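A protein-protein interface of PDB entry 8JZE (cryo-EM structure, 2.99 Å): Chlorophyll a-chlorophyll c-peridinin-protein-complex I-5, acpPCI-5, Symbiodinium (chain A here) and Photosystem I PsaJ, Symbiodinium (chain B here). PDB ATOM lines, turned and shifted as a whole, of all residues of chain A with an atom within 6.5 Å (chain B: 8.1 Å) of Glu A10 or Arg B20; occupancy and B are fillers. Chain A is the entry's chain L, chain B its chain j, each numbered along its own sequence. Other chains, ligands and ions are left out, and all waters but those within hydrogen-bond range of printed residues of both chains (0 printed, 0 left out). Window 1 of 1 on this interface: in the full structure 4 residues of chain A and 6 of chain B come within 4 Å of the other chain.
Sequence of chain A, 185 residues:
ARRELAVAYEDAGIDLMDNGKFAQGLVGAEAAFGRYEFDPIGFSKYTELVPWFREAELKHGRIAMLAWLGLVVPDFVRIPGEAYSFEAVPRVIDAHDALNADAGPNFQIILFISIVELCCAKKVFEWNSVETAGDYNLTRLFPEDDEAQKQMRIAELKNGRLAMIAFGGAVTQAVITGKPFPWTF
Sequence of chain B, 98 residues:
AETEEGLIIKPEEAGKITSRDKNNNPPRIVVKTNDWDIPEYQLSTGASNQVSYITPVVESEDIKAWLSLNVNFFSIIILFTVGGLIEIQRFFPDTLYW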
ATOM      1  N   ARG A   3     -33.486  14.668 -19.818  1.00  0.00           N
ATOM      2  CA  ARG A   3     -33.172  13.712 -18.729  1.00  0.00           C
ATOM      3  C   ARG A   3     -32.433  14.445 -17.608  1.00  0.00           C
ATOM      4  O   ARG A   3     -31.534  15.238 -17.926  1.00  0.00           O
ATOM      5  CB  ARG A   3     -32.388  12.517 -19.282  1.00  0.00           C
ATOM      6  CG  ARG A   3     -32.800  11.180 -18.689  1.00  0.00           C
ATOM      7  CD  ARG A   3     -32.560  10.044 -19.661  1.00  0.00           C
ATOM      8  NE  ARG A   3     -31.360  10.249 -20.456  1.00  0.00           N
ATOM      9  CZ  ARG A   3     -30.335   9.409 -20.485  1.00  0.00           C
ATOM     10  NH1 ARG A   3     -30.362   8.307 -19.756  1.00  0.00           N
ATOM     11  NH2 ARG A   3     -29.284   9.673 -21.240  1.00  0.00           N
ATOM     12  N   LEU A   5     -29.822  15.199 -14.612  1.00  0.00           N
ATOM     13  CA  LEU A   5     -28.388  14.826 -14.487  1.00  0.00           C
ATOM     14  C   LEU A   5     -28.280  13.542 -13.658  1.00  0.00           C
ATOM     15  O   LEU A   5     -27.374  12.739 -13.936  1.00  0.00           O
ATOM     16  CB  LEU A   5     -27.632  15.979 -13.822  1.00  0.00           C
ATOM     17  CG  LEU A   5     -27.248  17.138 -14.742  1.00  0.00           C
ATOM     18  CD1 LEU A   5     -27.790  16.926 -16.148  1.00  0.00           C
ATOM     19  CD2 LEU A   5     -27.728  18.465 -14.179  1.00  0.00           C
ATOM     20  N   ALA A   6     -29.187  13.352 -12.694  1.00  0.00           N
ATOM     21  CA  ALA A   6     -29.139  12.159 -11.818  1.00  0.00           C
ATOM     22  C   ALA A   6     -29.091  10.889 -12.675  1.00  0.00           C
ATOM     23  O   ALA A   6     -28.305   9.980 -12.340  1.00  0.00           O
ATOM     24  CB  ALA A   6     -30.331  12.153 -10.893  1.00  0.00           C
ATOM     25  N   VAL A   7     -29.899  10.836 -13.738  1.00  0.00           N
ATOM     26  CA  VAL A   7     -29.923   9.646 -14.639  1.00  0.00           C
ATOM     27  C   VAL A   7     -29.102   9.966 -15.893  1.00  0.00           C
ATOM     28  O   VAL A   7     -28.292   9.112 -16.299  1.00  0.00           O
ATOM     29  CB  VAL A   7     -31.366   9.241 -14.994  1.00  0.00           C
ATOM     30  CG1 VAL A   7     -32.278  10.452 -15.117  1.00  0.00           C
ATOM     31  CG2 VAL A   7     -31.422   8.391 -16.254  1.00  0.00           C
ATOM     32  N   ALA A   8     -29.308  11.150 -16.477  1.00  0.00           N
ATOM     33  CA  ALA A   8     -28.547  11.552 -17.657  1.00  0.00           C
ATOM     34  C   ALA A   8     -27.062  11.261 -17.493  1.00  0.00           C
ATOM     35  O   ALA A   8     -26.377  10.933 -18.468  1.00  0.00           O
ATOM     36  CB  ALA A   8     -28.763  13.037 -17.947  1.00  0.00           C
ATOM     37  N   TYR A   9     -26.543  11.383 -16.270  1.00  0.00           N
ATOM     38  CA  TYR A   9     -25.120  11.158 -16.042  1.00  0.00           C
ATOM     39  C   TYR A   9     -24.713   9.710 -16.275  1.00  0.00           C
ATOM     40  O   TYR A   9     -23.516   9.430 -16.405  1.00  0.00           O
ATOM     41  CB  TYR A   9     -24.738  11.581 -14.621  1.00  0.00           C
ATOM     42  CG  TYR A   9     -24.556  13.072 -14.453  1.00  0.00           C
ATOM     43  CD1 TYR A   9     -24.617  13.926 -15.546  1.00  0.00           C
ATOM     44  CD2 TYR A   9     -24.312  13.623 -13.204  1.00  0.00           C
ATOM     45  CE1 TYR A   9     -24.449  15.284 -15.398  1.00  0.00           C
ATOM     46  CE2 TYR A   9     -24.141  14.980 -13.046  1.00  0.00           C
ATOM     47  CZ  TYR A   9     -24.210  15.807 -14.147  1.00  0.00           C
ATOM     48  OH  TYR A   9     -24.041  17.163 -14.001  1.00  0.00           O
ATOM     49  N   GLU A  10     -25.673   8.786 -16.337  1.00  0.00           N
ATOM     50  CA  GLU A  10     -25.344   7.384 -16.566  1.00  0.00           C
ATOM     51  C   GLU A  10     -24.904   7.104 -17.998  1.00  0.00           C
ATOM     52  O   GLU A  10     -24.378   6.018 -18.260  1.00  0.00           O
ATOM     53  CB  GLU A  10     -26.536   6.498 -16.203  1.00  0.00           C
ATOM     54  CG  GLU A  10     -26.864   6.486 -14.717  1.00  0.00           C
ATOM     55  CD  GLU A  10     -27.883   5.426 -14.349  1.00  0.00           C
ATOM     56  OE1 GLU A  10     -28.760   5.122 -15.185  1.00  0.00           O
ATOM     57  OE2 GLU A  10     -27.805   4.891 -13.224  1.00  0.00           O
ATOM     58  N   ASP A  11     -25.105   8.045 -18.921  1.00  0.00           N
ATOM     59  CA  ASP A  11     -24.650   7.906 -20.299  1.00  0.00           C
ATOM     60  C   ASP A  11     -23.613   8.968 -20.653  1.00  0.00           C
ATOM     61  O   ASP A  11     -23.483   9.355 -21.816  1.00  0.00           O
ATOM     62  CB  ASP A  11     -25.827   7.968 -21.272  1.00  0.00           C
ATOM     63  CG  ASP A  11     -26.706   6.733 -21.209  1.00  0.00           C
ATOM     64  OD1 ASP A  11     -26.567   5.947 -20.249  1.00  0.00           O
ATOM     65  OD2 ASP A  11     -27.530   6.543 -22.129  1.00  0.00           O
ATOM     66  N   ALA A  12     -22.868   9.443 -19.662  1.00  0.00           N
ATOM     67  CA  ALA A  12     -21.848  10.460 -19.864  1.00  0.00           C
ATOM     68  C   ALA A  12     -20.489   9.814 -20.118  1.00  0.00           C
ATOM     69  O   ALA A  12     -20.287   8.618 -19.905  1.00  0.00           O
ATOM     70  CB  ALA A  12     -21.780  11.401 -18.657  1.00  0.00           C
ATOM     71  N   TRP A 127     -18.807  13.645 -16.518  1.00  0.00           N
ATOM     72  CA  TRP A 127     -20.243  13.916 -16.460  1.00  0.00           C
ATOM     73  C   TRP A 127     -20.725  14.808 -17.600  1.00  0.00           C
ATOM     74  O   TRP A 127     -21.893  15.204 -17.627  1.00  0.00           O
ATOM     75  CB  TRP A 127     -20.614  14.548 -15.114  1.00  0.00           C
ATOM     76  CG  TRP A 127     -20.052  13.811 -13.946  1.00  0.00           C
ATOM     77  CD1 TRP A 127     -19.184  14.291 -13.010  1.00  0.00           C
ATOM     78  CD2 TRP A 127     -20.304  12.445 -13.599  1.00  0.00           C
ATOM     79  NE1 TRP A 127     -18.886  13.309 -12.095  1.00  0.00           N
ATOM     80  CE2 TRP A 127     -19.561  12.166 -12.438  1.00  0.00           C
ATOM     81  CE3 TRP A 127     -21.089  11.434 -14.157  1.00  0.00           C
ATOM     82  CZ2 TRP A 127     -19.578  10.915 -11.825  1.00  0.00           C
ATOM     83  CZ3 TRP A 127     -21.106  10.195 -13.548  1.00  0.00           C
ATOM     84  CH2 TRP A 127     -20.358   9.946 -12.394  1.00  0.00           C
ATOM     85  N   GLU B   5     -16.354  -3.434  -4.673  1.00  0.00           N
ATOM     86  CA  GLU B   5     -17.512  -3.236  -5.544  1.00  0.00           C
ATOM     87  C   GLU B   5     -17.065  -2.435  -6.765  1.00  0.00           C
ATOM     88  O   GLU B   5     -17.042  -1.201  -6.739  1.00  0.00           O
ATOM     89  CB  GLU B   5     -18.648  -2.538  -4.800  1.00  0.00           C
ATOM     90  CG  GLU B   5     -18.229  -1.319  -3.982  1.00  0.00           C
ATOM     91  CD  GLU B   5     -17.734  -1.674  -2.596  1.00  0.00           C
ATOM     92  OE1 GLU B   5     -17.847  -2.855  -2.210  1.00  0.00           O
ATOM     93  OE2 GLU B   5     -17.235  -0.771  -1.893  1.00  0.00           O
ATOM     94  N   GLY B   6     -16.701  -3.135  -7.834  1.00  0.00           N
ATOM     95  CA  GLY B   6     -16.323  -2.456  -9.057  1.00  0.00           C
ATOM     96  C   GLY B   6     -16.963  -3.042 -10.297  1.00  0.00           C
ATOM     97  O   GLY B   6     -16.911  -2.435 -11.371  1.00  0.00           O
ATOM     98  N   LEU B   7     -17.584  -4.213 -10.153  1.00  0.00           N
ATOM     99  CA  LEU B   7     -18.089  -4.983 -11.288  1.00  0.00           C
ATOM    100  C   LEU B   7     -16.996  -5.156 -12.338  1.00  0.00           C
ATOM    101  O   LEU B   7     -17.199  -4.943 -13.535  1.00  0.00           O
ATOM    102  CB  LEU B   7     -19.342  -4.342 -11.886  1.00  0.00           C
ATOM    103  CG  LEU B   7     -20.669  -4.885 -11.354  1.00  0.00           C
ATOM    104  CD1 LEU B   7     -20.794  -6.372 -11.649  1.00  0.00           C
ATOM    105  CD2 LEU B   7     -20.812  -4.627  -9.862  1.00  0.00           C
ATOM    106  N   ILE B   8     -15.812  -5.539 -11.861  1.00  0.00           N
ATOM    107  CA  ILE B   8     -14.646  -5.663 -12.723  1.00  0.00           C
ATOM    108  C   ILE B   8     -14.873  -6.792 -13.720  1.00  0.00           C
ATOM    109  O   ILE B   8     -15.263  -7.905 -13.344  1.00  0.00           O
ATOM    110  CB  ILE B   8     -13.386  -5.905 -11.880  1.00  0.00           C
ATOM    111  CG1 ILE B   8     -13.398  -5.020 -10.632  1.00  0.00           C
ATOM    112  CG2 ILE B   8     -12.150  -5.616 -12.692  1.00  0.00           C
ATOM    113  CD1 ILE B   8     -13.174  -3.549 -10.917  1.00  0.00           C
ATOM    114  N   ILE B   9     -14.630  -6.508 -15.000  1.00  0.00           N
ATOM    115  CA  ILE B   9     -14.865  -7.466 -16.071  1.00  0.00           C
ATOM    116  C   ILE B   9     -13.620  -7.555 -16.944  1.00  0.00           C
ATOM    117  O   ILE B   9     -12.778  -6.656 -16.964  1.00  0.00           O
ATOM    118  CB  ILE B   9     -16.094  -7.099 -16.929  1.00  0.00           C
ATOM    119  CG1 ILE B   9     -15.900  -5.736 -17.589  1.00  0.00           C
ATOM    120  CG2 ILE B   9     -17.351  -7.104 -16.081  1.00  0.00           C
ATOM    121  CD1 ILE B   9     -17.046  -5.324 -18.484  1.00  0.00           C
ATOM    122  N   ILE B  17     -21.125  -7.231 -20.531  1.00  0.00           N
ATOM    123  CA  ILE B  17     -21.562  -6.949 -19.168  1.00  0.00           C
ATOM    124  C   ILE B  17     -21.999  -5.493 -19.079  1.00  0.00           C
ATOM    125  O   ILE B  17     -21.299  -4.591 -19.552  1.00  0.00           O
ATOM    126  CB  ILE B  17     -20.441  -7.256 -18.162  1.00  0.00           C
ATOM    127  CG1 ILE B  17     -19.944  -8.692 -18.336  1.00  0.00           C
ATOM    128  CG2 ILE B  17     -20.930  -7.031 -16.740  1.00  0.00           C
ATOM    129  CD1 ILE B  17     -21.005  -9.742 -18.096  1.00  0.00           C
ATOM    130  N   THR B  18     -23.164  -5.263 -18.475  1.00  0.00           N
ATOM    131  CA  THR B  18     -23.698  -3.916 -18.307  1.00  0.00           C
ATOM    132  C   THR B  18     -24.162  -3.605 -16.889  1.00  0.00           C
ATOM    133  O   THR B  18     -24.273  -2.421 -16.551  1.00  0.00           O
ATOM    134  CB  THR B  18     -24.866  -3.678 -19.279  1.00  0.00           C
ATOM    135  OG1 THR B  18     -24.544  -4.247 -20.554  1.00  0.00           O
ATOM    136  CG2 THR B  18     -25.124  -2.188 -19.468  1.00  0.00           C
ATOM    137  N   SER B  19     -24.434  -4.612 -16.058  1.00  0.00           N
ATOM    138  CA  SER B  19     -24.763  -4.386 -14.653  1.00  0.00           C
ATOM    139  C   SER B  19     -23.727  -3.475 -14.015  1.00  0.00           C
ATOM    140  O   SER B  19     -22.540  -3.811 -13.963  1.00  0.00           O
ATOM    141  CB  SER B  19     -24.829  -5.723 -13.912  1.00  0.00           C
ATOM    142  OG  SER B  19     -23.567  -6.369 -13.917  1.00  0.00           O
ATOM    143  N   ARG B  20     -24.176  -2.318 -13.530  1.00  0.00           N
ATOM    144  CA  ARG B  20     -23.238  -1.224 -13.276  1.00  0.00           C
ATOM    145  C   ARG B  20     -22.433  -1.431 -11.994  1.00  0.00           C
ATOM    146  O   ARG B  20     -21.226  -1.685 -12.047  1.00  0.00           O
ATOM    147  CB  ARG B  20     -24.000   0.105 -13.232  1.00  0.00           C
ATOM    148  CG  ARG B  20     -24.871   0.366 -14.456  1.00  0.00           C
ATOM    149  CD  ARG B  20     -25.581   1.712 -14.373  1.00  0.00           C
ATOM    150  NE  ARG B  20     -24.652   2.834 -14.439  1.00  0.00           N
ATOM    151  CZ  ARG B  20     -24.284   3.440 -15.560  1.00  0.00           C
ATOM    152  NH1 ARG B  20     -24.750   3.057 -16.737  1.00  0.00           N
ATOM    153  NH2 ARG B  20     -23.425   4.452 -15.497  1.00  0.00           N
ATOM    154  N   ASP B  21     -23.096  -1.372 -10.835  1.00  0.00           N
ATOM    155  CA  ASP B  21     -22.394  -1.380  -9.553  1.00  0.00           C
ATOM    156  C   ASP B  21     -23.366  -1.281  -8.384  1.00  0.00           C
ATOM    157  O   ASP B  21     -24.578  -1.158  -8.587  1.00  0.00           O
ATOM    158  CB  ASP B  21     -21.389  -0.227  -9.481  1.00  0.00           C
ATOM    159  CG  ASP B  21     -20.169  -0.566  -8.652  1.00  0.00           C
ATOM    160  OD1 ASP B  21     -20.156  -1.641  -8.018  1.00  0.00           O
ATOM    161  OD2 ASP B  21     -19.219   0.244  -8.642  1.00  0.00           O
ATOM    162  N   LYS B  22     -22.848  -1.345  -7.153  1.00  0.00           N
ATOM    163  CA  LYS B  22     -23.621  -0.844  -6.020  1.00  0.00           C
ATOM    164  C   LYS B  22     -23.795   0.666  -6.119  1.00  0.00           C
ATOM    165  O   LYS B  22     -24.826   1.203  -5.698  1.00  0.00           O
ATOM    166  CB  LYS B  22     -22.958  -1.239  -4.696  1.00  0.00           C
ATOM    167  CG  LYS B  22     -21.641  -0.537  -4.391  1.00  0.00           C
ATOM    168  CD  LYS B  22     -21.826   0.604  -3.397  1.00  0.00           C
ATOM    169  CE  LYS B  22     -20.508   1.300  -3.092  1.00  0.00           C
ATOM    170  NZ  LYS B  22     -20.689   2.468  -2.186  1.00  0.00           N
ATOM    171  N   ASN B  23     -22.794   1.358  -6.658  1.00  0.00           N
ATOM    172  CA  ASN B  23     -22.961   2.706  -7.181  1.00  0.00           C
ATOM    173  C   ASN B  23     -23.560   2.588  -8.582  1.00  0.00           C
ATOM    174  O   ASN B  23     -24.047   1.528  -8.983  1.00  0.00           O
ATOM    175  CB  ASN B  23     -21.627   3.450  -7.180  1.00  0.00           C
ATOM    176  CG  ASN B  23     -21.007   3.542  -5.799  1.00  0.00           C
ATOM    177  OD1 ASN B  23     -21.696   3.786  -4.810  1.00  0.00           O
ATOM    178  ND2 ASN B  23     -19.696   3.347  -5.727  1.00  0.00           N
ATOM    179  N   ASN B  24     -23.549   3.673  -9.350  1.00  0.00           N
ATOM    180  CA  ASN B  24     -23.990   3.612 -10.738  1.00  0.00           C
ATOM    181  C   ASN B  24     -22.821   3.658 -11.717  1.00  0.00           C
ATOM    182  O   ASN B  24     -23.022   3.934 -12.903  1.00  0.00           O
ATOM    183  CB  ASN B  24     -24.988   4.731 -11.031  1.00  0.00           C
ATOM    184  CG  ASN B  24     -26.336   4.483 -10.391  1.00  0.00           C
ATOM    185  OD1 ASN B  24     -26.435   3.805  -9.370  1.00  0.00           O
ATOM    186  ND2 ASN B  24     -27.385   5.025 -10.995  1.00  0.00           N
ATOM    187  N   ASN B  25     -21.611   3.398 -11.242  1.00  0.00           N
ATOM    188  CA  ASN B  25     -20.448   3.380 -12.120  1.00  0.00           C
ATOM    189  C   ASN B  25     -20.533   2.197 -13.079  1.00  0.00           C
ATOM    190  O   ASN B  25     -20.847   1.081 -12.650  1.00  0.00           O
ATOM    191  CB  ASN B  25     -19.163   3.301 -11.299  1.00  0.00           C
ATOM    192  CG  ASN B  25     -18.981   4.495 -10.388  1.00  0.00           C
ATOM    193  OD1 ASN B  25     -19.501   5.576 -10.658  1.00  0.00           O
ATOM    194  ND2 ASN B  25     -18.239   4.309  -9.304  1.00  0.00           N
ATOM    195  N   PRO B  26     -20.261   2.393 -14.366  1.00  0.00           N
ATOM    196  CA  PRO B  26     -20.277   1.274 -15.312  1.00  0.00           C
ATOM    197  C   PRO B  26     -19.134   0.316 -15.033  1.00  0.00           C
ATOM    198  O   PRO B  26     -18.164   0.681 -14.351  1.00  0.00           O
ATOM    199  CB  PRO B  26     -20.114   1.965 -16.675  1.00  0.00           C
ATOM    200  CG  PRO B  26     -19.440   3.254 -16.366  1.00  0.00           C
ATOM    201  CD  PRO B  26     -19.971   3.676 -15.028  1.00  0.00           C
ATOM    202  N   PRO B  27     -19.212  -0.923 -15.526  1.00  0.00           N
ATOM    203  CA  PRO B  27     -18.144  -1.890 -15.247  1.00  0.00           C
ATOM    204  C   PRO B  27     -16.804  -1.427 -15.798  1.00  0.00           C
ATOM    205  O   PRO B  27     -16.727  -0.747 -16.823  1.00  0.00           O
ATOM    206  CB  PRO B  27     -18.627  -3.167 -15.945  1.00  0.00           C
ATOM    207  CG  PRO B  27     -19.588  -2.694 -16.982  1.00  0.00           C
ATOM    208  CD  PRO B  27     -20.267  -1.506 -16.372  1.00  0.00           C
ATOM    209  N   ARG B  28     -15.741  -1.803 -15.095  1.00  0.00           N
ATOM    210  CA  ARG B  28     -14.384  -1.424 -15.460  1.00  0.00           C
ATOM    211  C   ARG B  28     -13.641  -2.619 -16.044  1.00  0.00           C
ATOM    212  O   ARG B  28     -13.717  -3.731 -15.515  1.00  0.00           O
ATOM    213  CB  ARG B  28     -13.622  -0.882 -14.248  1.00  0.00           C
ATOM    214  CG  ARG B  28     -14.268   0.327 -13.592  1.00  0.00           C
ATOM    215  CD  ARG B  28     -13.463   0.806 -12.394  1.00  0.00           C
ATOM    216  NE  ARG B  28     -12.097   1.160 -12.760  1.00  0.00           N
ATOM    217  CZ  ARG B  28     -11.723   2.355 -13.195  1.00  0.00           C
ATOM    218  NH1 ARG B  28     -12.590   3.344 -13.332  1.00  0.00           N
ATOM    219  NH2 ARG B  28     -10.445   2.563 -13.502  1.00  0.00           N
ATOM    220  N   THR B  45     -15.527   2.364 -18.608  1.00  0.00           N
ATOM    221  CA  THR B  45     -16.480   2.268 -19.703  1.00  0.00           C
ATOM    222  C   THR B  45     -17.346   3.513 -19.832  1.00  0.00           C
ATOM    223  O   THR B  45     -18.063   3.657 -20.829  1.00  0.00           O
ATOM    224  CB  THR B  45     -17.370   1.026 -19.510  1.00  0.00           C
ATOM    225  OG1 THR B  45     -16.551  -0.088 -19.136  1.00  0.00           O
ATOM    226  CG2 THR B  45     -18.113   0.669 -20.788  1.00  0.00           C
ATOM    227  N   GLY B  46     -17.286   4.419 -18.867  1.00  0.00           N
ATOM    228  CA  GLY B  46     -18.041   5.650 -18.950  1.00  0.00           C
ATOM    229  C   GLY B  46     -17.705   6.555 -17.787  1.00  0.00           C
ATOM    230  O   GLY B  46     -16.753   6.312 -17.043  1.00  0.00           O
ATOM    231  N   ALA B  47     -18.501   7.611 -17.642  1.00  0.00           N
ATOM    232  CA  ALA B  47     -18.333   8.508 -16.508  1.00  0.00           C
ATOM    233  C   ALA B  47     -18.612   7.765 -15.208  1.00  0.00           C
ATOM    234  O   ALA B  47     -19.540   6.957 -15.123  1.00  0.00           O
ATOM    235  CB  ALA B  47     -19.260   9.713 -16.640  1.00  0.00           C
ATOM    236  N   SER B  48     -17.799   8.039 -14.192  1.00  0.00           N
ATOM    237  CA  SER B  48     -17.917   7.335 -12.924  1.00  0.00           C
ATOM    238  C   SER B  48     -17.255   8.152 -11.825  1.00  0.00           C
ATOM    239  O   SER B  48     -16.236   8.806 -12.060  1.00  0.00           O
ATOM    240  CB  SER B  48     -17.275   5.946 -13.008  1.00  0.00           C
ATOM    241  OG  SER B  48     -15.897   6.039 -13.325  1.00  0.00           O
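The guanidinium group (NE) of Arg B20 is in salt-bridge range of the side-chain carboxylate (OE2) of Glu A10, at 3.96 Å.
The backbone NH (N) of Ala B47 lies within hydrogen-bond range of the backbone carbonyl oxygen (O) of Ala A12.
The side-chain amide nitrogen (ND2) of Asn B24 sits close to the side-chain carboxylate (OE2) of Glu A10 (2.3 Å).
The guanidinium group of Arg B20 lies within hydrogen-bond range of the backbone carbonyl oxygen of Asn B24.
Among the printed residues, merely in contact across the chains: Ala A12 with Gly B46 (3.8 Å), Trp A127 with Ala B47 (3.5 Å) and Trp A127 with Ser B48 (3.6 Å).
Of chain B, only Arg B20 and Asn B24 come within 4 Å of Glu A10.
Of the printed residues of chain B, Ala A12 touches Gly B46 (3.8 Å) and Ala B47 (3.1 Å).
Of chain A, only Glu A10 (3.3 Å) comes within 4 Å of Arg B20.
Of the printed residues of chain A, Asn B24 touches Glu A10.
Of the printed residues of chain A, Gly B46 touches Ala A12 (3.8 Å).
The nearest residue of chain B that does not touch Glu A10 is Ala B47 (5.8 Å).
The nearest printed residue of chain A that does not touch Asn B24 is Ala A6 (5.2 Å).
Of the 21 printed residues of chain B, 5 touch a printed residue of chain A.
Along chain A the printed residues that touch a printed residue of chain B span positions 10 to 127.
Among the printed residues, 6 pairs touch across the chains.
Among the printed residues, Asp or Glu carboxylates within 4 Å of a Lys or Arg side-chain nitrogen of the other chain: Glu A10 with Arg B20 (3.96 Å).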
